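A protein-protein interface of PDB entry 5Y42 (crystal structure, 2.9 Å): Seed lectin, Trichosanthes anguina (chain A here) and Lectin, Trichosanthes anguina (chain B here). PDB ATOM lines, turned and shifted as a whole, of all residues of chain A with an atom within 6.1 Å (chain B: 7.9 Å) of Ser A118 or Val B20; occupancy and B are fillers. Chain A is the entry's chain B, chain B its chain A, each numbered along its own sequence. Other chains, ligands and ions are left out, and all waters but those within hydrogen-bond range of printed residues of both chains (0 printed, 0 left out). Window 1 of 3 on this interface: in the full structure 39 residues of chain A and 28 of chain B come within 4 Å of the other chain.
The guanidinium group (NH1) of Arg B21 is in salt-bridge range of the side-chain carboxylate (OE1) of Glu A124 (2.9 Å).
The side-chain hydroxyl of Tyr B13 lies within hydrogen-bond range of the backbone carbonyl oxygen of Met A113, at 2.6 Å.
OE2 of Glu B23 is in hydrogen-bond range of OH of Tyr A4 (3.2 Å).
NH2 of Arg B21 is in hydrogen-bond range of O of Ala A117 (2.7 Å).
The guanidinium group (NE) of Arg B21 is in hydrogen-bond range of the backbone carbonyl oxygen (O) of Ser A118.
N of Ala A196 is in hydrogen-bond range of O of Lys A119, 2.8 Å away.
NZ of Lys B38 is in hydrogen-bond range of O of Gly B25, at 2.8 Å.
The backbone carbonyl oxygen (O) of Glu B23 is in hydrogen-bond range of the side-chain amino group (NZ) of Lys B38 (2.8 Å).
O of Gln A112 sits at hydrogen-bond distance from N of Ala A117 (3.1 Å).
The backbone carbonyl oxygen (O) of Leu B24 lies within hydrogen-bond range of the backbone NH (N) of Lys B38 (2.9 Å).
The guanidinium group of Arg B19 lies within salt-bridge range of the side-chain carboxylate of Glu B23 (3.2 Å).
Tyr A4 touches Leu B41.
Met A25 touches Leu B37.
Phe B16 touches Val A114 (CE2 to CG1, 3.9 Å).
Ile B17 touches Val A114.
OH of Tyr B13 touches CB of Ala A117 (3.1 Å).
NH2 of Arg B21 touches O of Phe A120, 3.6 Å away.
Glu A124 touches Tyr B13.
OE2 of Glu A124 touches CG of Lys B14, 3.6 Å away.
OE2 of Glu A124 touches CG2 of Ile B17 (3.8 Å).
CB of Ala A196 touches NE of Arg B21, 3.7 Å away.
Ser A118 touches just these residues of chain B: Ile B17 (3.6 Å), Val B20 (3.4 Å) and Arg B21 (2.9 Å).
Val B20 touches just one residue of chain A: Ser A118 (3.4 Å).
Printed residues of chain A within 4 Å of Ile B17: Val A114 (3.6 Å), Ala A117 (3.97 Å), Ser A118 (3.6 Å) and Glu A124 (3.8 Å).
Of the printed residues of chain B, Phe A120 touches Arg B21 (3.6 Å).
Of the printed residues of chain B, Met A113 touches Tyr B13.
Lys A119 touches none of the printed residues of chain B.
The nearest printed residue of chain B that does not touch Ser A118 is Tyr B13 (5.8 Å).
Printed residues of chain A that touch a printed residue of chain B: Tyr A4, Leu A6, Met A25, Met A113, Val A114, Ala A117, Ser A118, Phe A120, Glu A124, Ala A196 and Leu A197.
Hydrophobic or aromatic side chains of chain A within 4 Å of the printed part of chain B: Tyr A4, Met A25, Val A114, Ala A117, Ala A196 and Leu A197.
Hydrophobic or aromatic side chains of chain B within 4 Å of the printed part of chain A: Ala B1, Tyr B13, Phe B16, Ile B17, Val B20, Leu B24, Leu B37 and Leu B41.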
ATOM      1  N   TYR A   4     -17.980  -5.373   2.336  1.00  0.00           N
ATOM      2  CA  TYR A   4     -17.997  -6.794   2.064  1.00  0.00           C
ATOM      3  C   TYR A   4     -16.627  -7.131   1.498  1.00  0.00           C
ATOM      4  O   TYR A   4     -16.255  -6.527   0.471  1.00  0.00           O
ATOM      5  CB  TYR A   4     -19.084  -7.077   1.045  1.00  0.00           C
ATOM      6  CG  TYR A   4     -19.227  -8.510   0.646  1.00  0.00           C
ATOM      7  CD1 TYR A   4     -19.540  -9.491   1.587  1.00  0.00           C
ATOM      8  CD2 TYR A   4     -19.121  -8.883  -0.691  1.00  0.00           C
ATOM      9  CE1 TYR A   4     -19.705 -10.811   1.215  1.00  0.00           C
ATOM     10  CE2 TYR A   4     -19.305 -10.200  -1.081  1.00  0.00           C
ATOM     11  CZ  TYR A   4     -19.588 -11.166  -0.128  1.00  0.00           C
ATOM     12  OH  TYR A   4     -19.741 -12.484  -0.522  1.00  0.00           O
ATOM     13  N   LEU A   6     -13.963 -10.140   0.166  1.00  0.00           N
ATOM     14  CA  LEU A   6     -14.136 -10.911  -1.036  1.00  0.00           C
ATOM     15  C   LEU A   6     -12.757 -11.253  -1.467  1.00  0.00           C
ATOM     16  O   LEU A   6     -11.921 -10.383  -1.440  1.00  0.00           O
ATOM     17  CB  LEU A   6     -14.899 -10.090  -2.084  1.00  0.00           C
ATOM     18  CG  LEU A   6     -15.394 -10.586  -3.428  1.00  0.00           C
ATOM     19  CD1 LEU A   6     -16.702  -9.859  -3.700  1.00  0.00           C
ATOM     20  CD2 LEU A   6     -14.350 -10.315  -4.511  1.00  0.00           C
ATOM     21  N   MET A  25     -22.427  -0.724  -4.035  1.00  0.00           N
ATOM     22  CA  MET A  25     -21.701  -1.798  -4.688  1.00  0.00           C
ATOM     23  C   MET A  25     -20.554  -1.365  -5.595  1.00  0.00           C
ATOM     24  O   MET A  25     -20.512  -1.661  -6.776  1.00  0.00           O
ATOM     25  CB  MET A  25     -22.717  -2.600  -5.463  1.00  0.00           C
ATOM     26  CG  MET A  25     -22.314  -4.020  -5.710  1.00  0.00           C
ATOM     27  SD  MET A  25     -23.715  -4.734  -6.542  1.00  0.00           S
ATOM     28  CE  MET A  25     -22.953  -6.251  -7.093  1.00  0.00           C
ATOM     29  N   GLN A 112     -15.734  -5.395 -13.777  1.00  0.00           N
ATOM     30  CA  GLN A 112     -16.728  -5.881 -14.744  1.00  0.00           C
ATOM     31  C   GLN A 112     -17.046  -7.361 -14.555  1.00  0.00           C
ATOM     32  O   GLN A 112     -18.189  -7.742 -14.530  1.00  0.00           O
ATOM     33  CB  GLN A 112     -16.310  -5.552 -16.186  1.00  0.00           C
ATOM     34  CG  GLN A 112     -16.369  -4.085 -16.552  1.00  0.00           C
ATOM     35  CD  GLN A 112     -15.936  -3.870 -17.986  1.00  0.00           C
ATOM     36  OE1 GLN A 112     -14.744  -3.875 -18.287  1.00  0.00           O
ATOM     37  NE2 GLN A 112     -16.900  -3.700 -18.886  1.00  0.00           N
ATOM     38  N   MET A 113     -16.015  -8.173 -14.383  1.00  0.00           N
ATOM     39  CA  MET A 113     -16.193  -9.616 -14.310  1.00  0.00           C
ATOM     40  C   MET A 113     -16.749 -10.098 -12.977  1.00  0.00           C
ATOM     41  O   MET A 113     -17.212 -11.218 -12.882  1.00  0.00           O
ATOM     42  CB  MET A 113     -14.864 -10.333 -14.571  1.00  0.00           C
ATOM     43  CG  MET A 113     -14.341 -10.156 -15.990  1.00  0.00           C
ATOM     44  SD  MET A 113     -12.868 -11.150 -16.397  1.00  0.00           S
ATOM     45  CE  MET A 113     -13.581 -12.775 -16.519  1.00  0.00           C
ATOM     46  N   VAL A 114     -16.715  -9.249 -11.943  1.00  0.00           N
ATOM     47  CA  VAL A 114     -17.261  -9.621 -10.643  1.00  0.00           C
ATOM     48  C   VAL A 114     -18.489  -8.791 -10.263  1.00  0.00           C
ATOM     49  O   VAL A 114     -19.577  -9.342 -10.035  1.00  0.00           O
ATOM     50  CB  VAL A 114     -16.204  -9.503  -9.522  1.00  0.00           C
ATOM     51  CG1 VAL A 114     -16.813  -9.842  -8.167  1.00  0.00           C
ATOM     52  CG2 VAL A 114     -15.015 -10.417  -9.795  1.00  0.00           C
ATOM     53  N   LEU A 115     -18.339  -7.474 -10.216  1.00  0.00           N
ATOM     54  CA  LEU A 115     -19.418  -6.634  -9.713  1.00  0.00           C
ATOM     55  C   LEU A 115     -20.488  -6.410 -10.752  1.00  0.00           C
ATOM     56  O   LEU A 115     -21.666  -6.580 -10.465  1.00  0.00           O
ATOM     57  CB  LEU A 115     -18.854  -5.312  -9.191  1.00  0.00           C
ATOM     58  CG  LEU A 115     -17.830  -5.456  -8.052  1.00  0.00           C
ATOM     59  CD1 LEU A 115     -17.228  -4.104  -7.721  1.00  0.00           C
ATOM     60  CD2 LEU A 115     -18.419  -6.071  -6.794  1.00  0.00           C
ATOM     61  N   GLU A 116     -20.085  -6.099 -11.981  1.00  0.00           N
ATOM     62  CA  GLU A 116     -21.072  -5.843 -13.043  1.00  0.00           C
ATOM     63  C   GLU A 116     -21.806  -7.123 -13.485  1.00  0.00           C
ATOM     64  O   GLU A 116     -22.979  -7.149 -13.726  1.00  0.00           O
ATOM     65  CB  GLU A 116     -20.436  -5.106 -14.226  1.00  0.00           C
ATOM     66  CG  GLU A 116     -19.812  -3.759 -13.859  1.00  0.00           C
ATOM     67  CD  GLU A 116     -20.752  -2.787 -13.101  1.00  0.00           C
ATOM     68  OE1 GLU A 116     -21.682  -2.150 -13.678  1.00  0.00           O
ATOM     69  OE2 GLU A 116     -20.548  -2.634 -11.884  1.00  0.00           O
ATOM     70  N   ALA A 117     -21.088  -8.214 -13.458  1.00  0.00           N
ATOM     71  CA  ALA A 117     -21.606  -9.568 -13.647  1.00  0.00           C
ATOM     72  C   ALA A 117     -22.629  -9.939 -12.575  1.00  0.00           C
ATOM     73  O   ALA A 117     -23.642 -10.575 -12.871  1.00  0.00           O
ATOM     74  CB  ALA A 117     -20.446 -10.541 -13.694  1.00  0.00           C
ATOM     75  N   SER A 118     -22.367  -9.513 -11.344  1.00  0.00           N
ATOM     76  CA  SER A 118     -23.313  -9.807 -10.256  1.00  0.00           C
ATOM     77  C   SER A 118     -24.602  -9.011 -10.429  1.00  0.00           C
ATOM     78  O   SER A 118     -25.659  -9.412  -9.976  1.00  0.00           O
ATOM     79  CB  SER A 118     -22.690  -9.508  -8.898  1.00  0.00           C
ATOM     80  OG  SER A 118     -21.633 -10.403  -8.628  1.00  0.00           O
ATOM     81  N   LYS A 119     -24.496  -7.830 -11.033  1.00  0.00           N
ATOM     82  CA  LYS A 119     -25.665  -6.956 -11.194  1.00  0.00           C
ATOM     83  C   LYS A 119     -26.573  -7.421 -12.326  1.00  0.00           C
ATOM     84  O   LYS A 119     -27.766  -7.175 -12.277  1.00  0.00           O
ATOM     85  CB  LYS A 119     -25.171  -5.556 -11.562  1.00  0.00           C
ATOM     86  CG  LYS A 119     -24.551  -4.781 -10.414  1.00  0.00           C
ATOM     87  CD  LYS A 119     -23.849  -3.520 -10.890  1.00  0.00           C
ATOM     88  CE  LYS A 119     -23.266  -2.764  -9.714  1.00  0.00           C
ATOM     89  NZ  LYS A 119     -22.637  -1.497 -10.182  1.00  0.00           N
ATOM     90  N   PHE A 120     -25.968  -7.896 -13.408  1.00  0.00           N
ATOM     91  CA  PHE A 120     -26.697  -8.297 -14.605  1.00  0.00           C
ATOM     92  C   PHE A 120     -26.444  -9.710 -15.091  1.00  0.00           C
ATOM     93  O   PHE A 120     -25.313 -10.151 -15.168  1.00  0.00           O
ATOM     94  CB  PHE A 120     -26.339  -7.366 -15.759  1.00  0.00           C
ATOM     95  CG  PHE A 120     -26.698  -5.936 -15.529  1.00  0.00           C
ATOM     96  CD1 PHE A 120     -27.995  -5.516 -15.647  1.00  0.00           C
ATOM     97  CD2 PHE A 120     -25.731  -5.010 -15.225  1.00  0.00           C
ATOM     98  CE1 PHE A 120     -28.332  -4.202 -15.447  1.00  0.00           C
ATOM     99  CE2 PHE A 120     -26.056  -3.693 -15.023  1.00  0.00           C
ATOM    100  CZ  PHE A 120     -27.361  -3.290 -15.134  1.00  0.00           C
ATOM    101  N   ARG A 121     -27.513 -10.421 -15.415  1.00  0.00           N
ATOM    102  CA  ARG A 121     -27.389 -11.763 -15.944  1.00  0.00           C
ATOM    103  C   ARG A 121     -26.707 -11.773 -17.301  1.00  0.00           C
ATOM    104  O   ARG A 121     -25.919 -12.659 -17.597  1.00  0.00           O
ATOM    105  CB  ARG A 121     -28.741 -12.460 -15.993  1.00  0.00           C
ATOM    106  CG  ARG A 121     -29.213 -12.875 -14.620  1.00  0.00           C
ATOM    107  CD  ARG A 121     -30.388 -13.822 -14.656  1.00  0.00           C
ATOM    108  NE  ARG A 121     -30.783 -14.143 -13.294  1.00  0.00           N
ATOM    109  CZ  ARG A 121     -31.912 -13.748 -12.726  1.00  0.00           C
ATOM    110  NH1 ARG A 121     -32.788 -13.034 -13.405  1.00  0.00           N
ATOM    111  NH2 ARG A 121     -32.167 -14.081 -11.476  1.00  0.00           N
ATOM    112  N   ILE A 123     -24.350  -9.984 -18.370  1.00  0.00           N
ATOM    113  CA  ILE A 123     -22.906  -9.862 -18.210  1.00  0.00           C
ATOM    114  C   ILE A 123     -22.352 -11.121 -17.597  1.00  0.00           C
ATOM    115  O   ILE A 123     -21.333 -11.622 -18.012  1.00  0.00           O
ATOM    116  CB  ILE A 123     -22.532  -8.675 -17.336  1.00  0.00           C
ATOM    117  CG1 ILE A 123     -23.037  -7.390 -17.997  1.00  0.00           C
ATOM    118  CG2 ILE A 123     -21.016  -8.613 -17.158  1.00  0.00           C
ATOM    119  CD1 ILE A 123     -22.948  -6.141 -17.129  1.00  0.00           C
ATOM    120  N   GLU A 124     -23.017 -11.643 -16.585  1.00  0.00           N
ATOM    121  CA  GLU A 124     -22.657 -12.944 -16.049  1.00  0.00           C
ATOM    122  C   GLU A 124     -22.511 -13.988 -17.147  1.00  0.00           C
ATOM    123  O   GLU A 124     -21.522 -14.724 -17.186  1.00  0.00           O
ATOM    124  CB  GLU A 124     -23.703 -13.454 -15.068  1.00  0.00           C
ATOM    125  CG  GLU A 124     -23.253 -14.688 -14.270  1.00  0.00           C
ATOM    126  CD  GLU A 124     -24.388 -15.406 -13.538  1.00  0.00           C
ATOM    127  OE1 GLU A 124     -25.581 -15.032 -13.747  1.00  0.00           O
ATOM    128  OE2 GLU A 124     -24.088 -16.348 -12.754  1.00  0.00           O
ATOM    129  N   ALA A 196     -30.155  -8.320 -11.479  1.00  0.00           N
ATOM    130  CA  ALA A 196     -30.143  -9.245 -10.377  1.00  0.00           C
ATOM    131  C   ALA A 196     -29.958  -8.569  -9.032  1.00  0.00           C
ATOM    132  O   ALA A 196     -30.302  -9.147  -8.017  1.00  0.00           O
ATOM    133  CB  ALA A 196     -29.069 -10.300 -10.567  1.00  0.00           C
ATOM    134  N   LEU A 197     -29.368  -7.363  -9.008  1.00  0.00           N
ATOM    135  CA  LEU A 197     -29.310  -6.526  -7.847  1.00  0.00           C
ATOM    136  C   LEU A 197     -29.614  -5.109  -8.209  1.00  0.00           C
ATOM    137  O   LEU A 197     -29.129  -4.650  -9.218  1.00  0.00           O
ATOM    138  CB  LEU A 197     -27.886  -6.517  -7.312  1.00  0.00           C
ATOM    139  CG  LEU A 197     -27.395  -7.820  -6.703  1.00  0.00           C
ATOM    140  CD1 LEU A 197     -25.909  -7.710  -6.457  1.00  0.00           C
ATOM    141  CD2 LEU A 197     -28.124  -8.115  -5.394  1.00  0.00           C
ATOM    142  N   ALA B   1     -16.041 -15.447   0.686  1.00  0.00           N
ATOM    143  CA  ALA B   1     -16.428 -15.445  -0.765  1.00  0.00           C
ATOM    144  C   ALA B   1     -15.165 -15.373  -1.655  1.00  0.00           C
ATOM    145  O   ALA B   1     -14.660 -14.288  -1.984  1.00  0.00           O
ATOM    146  CB  ALA B   1     -17.395 -14.317  -1.073  1.00  0.00           C
ATOM    147  N   ASN B   2     -14.678 -16.564  -2.019  1.00  0.00           N
ATOM    148  CA  ASN B   2     -13.382 -16.776  -2.615  1.00  0.00           C
ATOM    149  C   ASN B   2     -13.625 -17.078  -4.098  1.00  0.00           C
ATOM    150  O   ASN B   2     -14.707 -17.527  -4.475  1.00  0.00           O
ATOM    151  CB  ASN B   2     -12.677 -17.945  -1.904  1.00  0.00           C
ATOM    152  CG  ASN B   2     -11.167 -17.911  -2.083  1.00  0.00           C
ATOM    153  OD1 ASN B   2     -10.677 -17.788  -3.203  1.00  0.00           O
ATOM    154  ND2 ASN B   2     -10.421 -18.024  -0.980  1.00  0.00           N
ATOM    155  N   TYR B  13     -17.446 -20.367 -11.572  1.00  0.00           N
ATOM    156  CA  TYR B  13     -17.652 -18.929 -11.761  1.00  0.00           C
ATOM    157  C   TYR B  13     -19.073 -18.503 -11.414  1.00  0.00           C
ATOM    158  O   TYR B  13     -19.262 -17.629 -10.579  1.00  0.00           O
ATOM    159  CB  TYR B  13     -17.306 -18.481 -13.175  1.00  0.00           C
ATOM    160  CG  TYR B  13     -17.671 -17.034 -13.427  1.00  0.00           C
ATOM    161  CD1 TYR B  13     -16.913 -15.994 -12.880  1.00  0.00           C
ATOM    162  CD2 TYR B  13     -18.786 -16.686 -14.196  1.00  0.00           C
ATOM    163  CE1 TYR B  13     -17.238 -14.656 -13.110  1.00  0.00           C
ATOM    164  CE2 TYR B  13     -19.119 -15.352 -14.429  1.00  0.00           C
ATOM    165  CZ  TYR B  13     -18.347 -14.349 -13.875  1.00  0.00           C
ATOM    166  OH  TYR B  13     -18.664 -13.044 -14.105  1.00  0.00           O
ATOM    167  N   LYS B  14     -20.072 -19.188 -11.971  1.00  0.00           N
ATOM    168  CA  LYS B  14     -21.508 -18.894 -11.721  1.00  0.00           C
ATOM    169  C   LYS B  14     -21.898 -19.068 -10.273  1.00  0.00           C
ATOM    170  O   LYS B  14     -22.707 -18.299  -9.751  1.00  0.00           O
ATOM    171  CB  LYS B  14     -22.373 -19.794 -12.650  1.00  0.00           C
ATOM    172  CG  LYS B  14     -22.417 -19.294 -14.103  1.00  0.00           C
ATOM    173  CD  LYS B  14     -22.848 -20.318 -15.173  1.00  0.00           C
ATOM    174  CE  LYS B  14     -24.348 -20.558 -15.196  1.00  0.00           C
ATOM    175  NZ  LYS B  14     -25.126 -19.346 -15.592  1.00  0.00           N
ATOM    176  N   THR B  15     -21.341 -20.093  -9.629  1.00  0.00           N
ATOM    177  CA  THR B  15     -21.557 -20.328  -8.198  1.00  0.00           C
ATOM    178  C   THR B  15     -21.040 -19.178  -7.347  1.00  0.00           C
ATOM    179  O   THR B  15     -21.685 -18.750  -6.387  1.00  0.00           O
ATOM    180  CB  THR B  15     -20.871 -21.642  -7.809  1.00  0.00           C
ATOM    181  OG1 THR B  15     -21.448 -22.739  -8.554  1.00  0.00           O
ATOM    182  CG2 THR B  15     -20.988 -21.866  -6.287  1.00  0.00           C
ATOM    183  N   PHE B  16     -19.838 -18.729  -7.674  1.00  0.00           N
ATOM    184  CA  PHE B  16     -19.218 -17.552  -7.040  1.00  0.00           C
ATOM    185  C   PHE B  16     -20.089 -16.294  -7.205  1.00  0.00           C
ATOM    186  O   PHE B  16     -20.397 -15.642  -6.227  1.00  0.00           O
ATOM    187  CB  PHE B  16     -17.793 -17.331  -7.601  1.00  0.00           C
ATOM    188  CG  PHE B  16     -17.202 -15.983  -7.277  1.00  0.00           C
ATOM    189  CD1 PHE B  16     -16.772 -15.706  -5.984  1.00  0.00           C
ATOM    190  CD2 PHE B  16     -17.058 -14.996  -8.254  1.00  0.00           C
ATOM    191  CE1 PHE B  16     -16.235 -14.473  -5.652  1.00  0.00           C
ATOM    192  CE2 PHE B  16     -16.521 -13.756  -7.933  1.00  0.00           C
ATOM    193  CZ  PHE B  16     -16.120 -13.491  -6.633  1.00  0.00           C
ATOM    194  N   ILE B  17     -20.486 -15.970  -8.436  1.00  0.00           N
ATOM    195  CA  ILE B  17     -21.357 -14.814  -8.684  1.00  0.00           C
ATOM    196  C   ILE B  17     -22.665 -14.994  -7.932  1.00  0.00           C
ATOM    197  O   ILE B  17     -23.213 -14.053  -7.349  1.00  0.00           O
ATOM    198  CB  ILE B  17     -21.633 -14.608 -10.181  1.00  0.00           C
ATOM    199  CG1 ILE B  17     -20.364 -14.140 -10.863  1.00  0.00           C
ATOM    200  CG2 ILE B  17     -22.753 -13.597 -10.455  1.00  0.00           C
ATOM    201  CD1 ILE B  17     -19.717 -12.955 -10.209  1.00  0.00           C
ATOM    202  N   GLY B  18     -23.147 -16.228  -7.911  1.00  0.00           N
ATOM    203  CA  GLY B  18     -24.366 -16.546  -7.152  1.00  0.00           C
ATOM    204  C   GLY B  18     -24.246 -16.242  -5.674  1.00  0.00           C
ATOM    205  O   GLY B  18     -25.151 -15.723  -5.088  1.00  0.00           O
ATOM    206  N   ARG B  19     -23.097 -16.565  -5.093  1.00  0.00           N
ATOM    207  CA  ARG B  19     -22.855 -16.263  -3.687  1.00  0.00           C
ATOM    208  C   ARG B  19     -22.709 -14.737  -3.414  1.00  0.00           C
ATOM    209  O   ARG B  19     -23.157 -14.226  -2.389  1.00  0.00           O
ATOM    210  CB  ARG B  19     -21.573 -16.982  -3.271  1.00  0.00           C
ATOM    211  CG  ARG B  19     -21.295 -16.958  -1.777  1.00  0.00           C
ATOM    212  CD  ARG B  19     -20.362 -18.081  -1.336  1.00  0.00           C
ATOM    213  NE  ARG B  19     -19.428 -17.671  -0.273  1.00  0.00           N
ATOM    214  CZ  ARG B  19     -19.776 -17.311   0.968  1.00  0.00           C
ATOM    215  NH1 ARG B  19     -21.058 -17.268   1.368  1.00  0.00           N
ATOM    216  NH2 ARG B  19     -18.821 -16.980   1.831  1.00  0.00           N
ATOM    217  N   VAL B  20     -22.058 -14.019  -4.321  1.00  0.00           N
ATOM    218  CA  VAL B  20     -21.927 -12.571  -4.167  1.00  0.00           C
ATOM    219  C   VAL B  20     -23.324 -11.951  -4.126  1.00  0.00           C
ATOM    220  O   VAL B  20     -23.620 -11.186  -3.228  1.00  0.00           O
ATOM    221  CB  VAL B  20     -21.070 -11.936  -5.275  1.00  0.00           C
ATOM    222  CG1 VAL B  20     -21.181 -10.410  -5.268  1.00  0.00           C
ATOM    223  CG2 VAL B  20     -19.623 -12.357  -5.105  1.00  0.00           C
ATOM    224  N   ARG B  21     -24.198 -12.334  -5.074  1.00  0.00           N
ATOM    225  CA  ARG B  21     -25.598 -11.887  -5.082  1.00  0.00           C
ATOM    226  C   ARG B  21     -26.336 -12.203  -3.808  1.00  0.00           C
ATOM    227  O   ARG B  21     -27.118 -11.379  -3.330  1.00  0.00           O
ATOM    228  CB  ARG B  21     -26.369 -12.513  -6.242  1.00  0.00           C
ATOM    229  CG  ARG B  21     -25.971 -11.993  -7.605  1.00  0.00           C
ATOM    230  CD  ARG B  21     -26.542 -12.829  -8.718  1.00  0.00           C
ATOM    231  NE  ARG B  21     -26.054 -12.278  -9.962  1.00  0.00           N
ATOM    232  CZ  ARG B  21     -26.176 -12.837 -11.158  1.00  0.00           C
ATOM    233  NH1 ARG B  21     -26.808 -13.990 -11.316  1.00  0.00           N
ATOM    234  NH2 ARG B  21     -25.663 -12.219 -12.212  1.00  0.00           N
ATOM    235  N   GLU B  22     -26.157 -13.403  -3.288  1.00  0.00           N
ATOM    236  CA  GLU B  22     -26.764 -13.841  -2.023  1.00  0.00           C
ATOM    237  C   GLU B  22     -26.455 -12.924  -0.827  1.00  0.00           C
ATOM    238  O   GLU B  22     -27.350 -12.534  -0.053  1.00  0.00           O
ATOM    239  CB  GLU B  22     -26.322 -15.320  -1.748  1.00  0.00           C
ATOM    240  CG  GLU B  22     -26.621 -15.922  -0.363  1.00  0.00           C
ATOM    241  CD  GLU B  22     -28.105 -15.908   0.025  1.00  0.00           C
ATOM    242  OE1 GLU B  22     -28.982 -15.803  -0.878  1.00  0.00           O
ATOM    243  OE2 GLU B  22     -28.402 -16.017   1.246  1.00  0.00           O
ATOM    244  N   GLU B  23     -25.140 -12.623  -0.725  1.00  0.00           N
ATOM    245  CA  GLU B  23     -24.601 -11.870   0.375  1.00  0.00           C
ATOM    246  C   GLU B  23     -24.932 -10.364   0.253  1.00  0.00           C
ATOM    247  O   GLU B  23     -25.114  -9.682   1.311  1.00  0.00           O
ATOM    248  CB  GLU B  23     -23.099 -12.066   0.478  1.00  0.00           C
ATOM    249  CG  GLU B  23     -22.698 -13.534   0.615  1.00  0.00           C
ATOM    250  CD  GLU B  23     -22.091 -13.880   1.960  1.00  0.00           C
ATOM    251  OE1 GLU B  23     -22.831 -13.926   2.963  1.00  0.00           O
ATOM    252  OE2 GLU B  23     -20.862 -14.103   2.004  1.00  0.00           O
ATOM    253  N   LEU B  24     -25.011  -9.824  -0.973  1.00  0.00           N
ATOM    254  CA  LEU B  24     -25.240  -8.391  -1.175  1.00  0.00           C
ATOM    255  C   LEU B  24     -26.743  -7.993  -1.334  1.00  0.00           C
ATOM    256  O   LEU B  24     -27.167  -6.885  -0.996  1.00  0.00           O
ATOM    257  CB  LEU B  24     -24.378  -7.841  -2.337  1.00  0.00           C
ATOM    258  CG  LEU B  24     -22.835  -7.970  -2.249  1.00  0.00           C
ATOM    259  CD1 LEU B  24     -22.130  -7.426  -3.494  1.00  0.00           C
ATOM    260  CD2 LEU B  24     -22.298  -7.265  -1.017  1.00  0.00           C
ATOM    261  N   GLY B  25     -27.534  -8.903  -1.858  1.00  0.00           N
ATOM    262  CA  GLY B  25     -28.939  -8.734  -2.033  1.00  0.00           C
ATOM    263  C   GLY B  25     -29.730  -9.022  -0.772  1.00  0.00           C
ATOM    264  O   GLY B  25     -29.449 -10.001  -0.046  1.00  0.00           O
ATOM    265  N   LEU B  37     -30.294  -3.889  -2.707  1.00  0.00           N
ATOM    266  CA  LEU B  37     -29.072  -4.082  -1.933  1.00  0.00           C
ATOM    267  C   LEU B  37     -29.355  -3.942  -0.448  1.00  0.00           C
ATOM    268  O   LEU B  37     -30.183  -3.121  -0.033  1.00  0.00           O
ATOM    269  CB  LEU B  37     -27.956  -3.113  -2.351  1.00  0.00           C
ATOM    270  CG  LEU B  37     -27.280  -3.390  -3.699  1.00  0.00           C
ATOM    271  CD1 LEU B  37     -26.560  -2.179  -4.265  1.00  0.00           C
ATOM    272  CD2 LEU B  37     -26.312  -4.554  -3.557  1.00  0.00           C
ATOM    273  N   LYS B  38     -28.663  -4.749   0.339  1.00  0.00           N
ATOM    274  CA  LYS B  38     -28.838  -4.782   1.788  1.00  0.00           C
ATOM    275  C   LYS B  38     -28.425  -3.478   2.415  1.00  0.00           C
ATOM    276  O   LYS B  38     -27.494  -2.846   1.941  1.00  0.00           O
ATOM    277  CB  LYS B  38     -27.945  -5.907   2.357  1.00  0.00           C
ATOM    278  CG  LYS B  38     -28.462  -7.330   2.175  1.00  0.00           C
ATOM    279  CD  LYS B  38     -27.964  -8.271   3.267  1.00  0.00           C
ATOM    280  CE  LYS B  38     -28.534  -9.673   3.135  1.00  0.00           C
ATOM    281  NZ  LYS B  38     -27.708 -10.420   2.148  1.00  0.00           N
ATOM    282  N   LEU B  41     -24.775  -5.922   6.534  1.00  0.00           N
ATOM    283  CA  LEU B  41     -24.381  -7.322   6.485  1.00  0.00           C
ATOM    284  C   LEU B  41     -24.371  -7.912   7.905  1.00  0.00           C
ATOM    285  O   LEU B  41     -23.769  -8.957   8.166  1.00  0.00           O
ATOM    286  CB  LEU B  41     -22.980  -7.395   5.846  1.00  0.00           C
ATOM    287  CG  LEU B  41     -22.831  -6.657   4.496  1.00  0.00           C
ATOM    288  CD1 LEU B  41     -21.409  -6.477   4.005  1.00  0.00           C
ATOM    289  CD2 LEU B  41     -23.614  -7.407   3.445  1.00  0.00           C
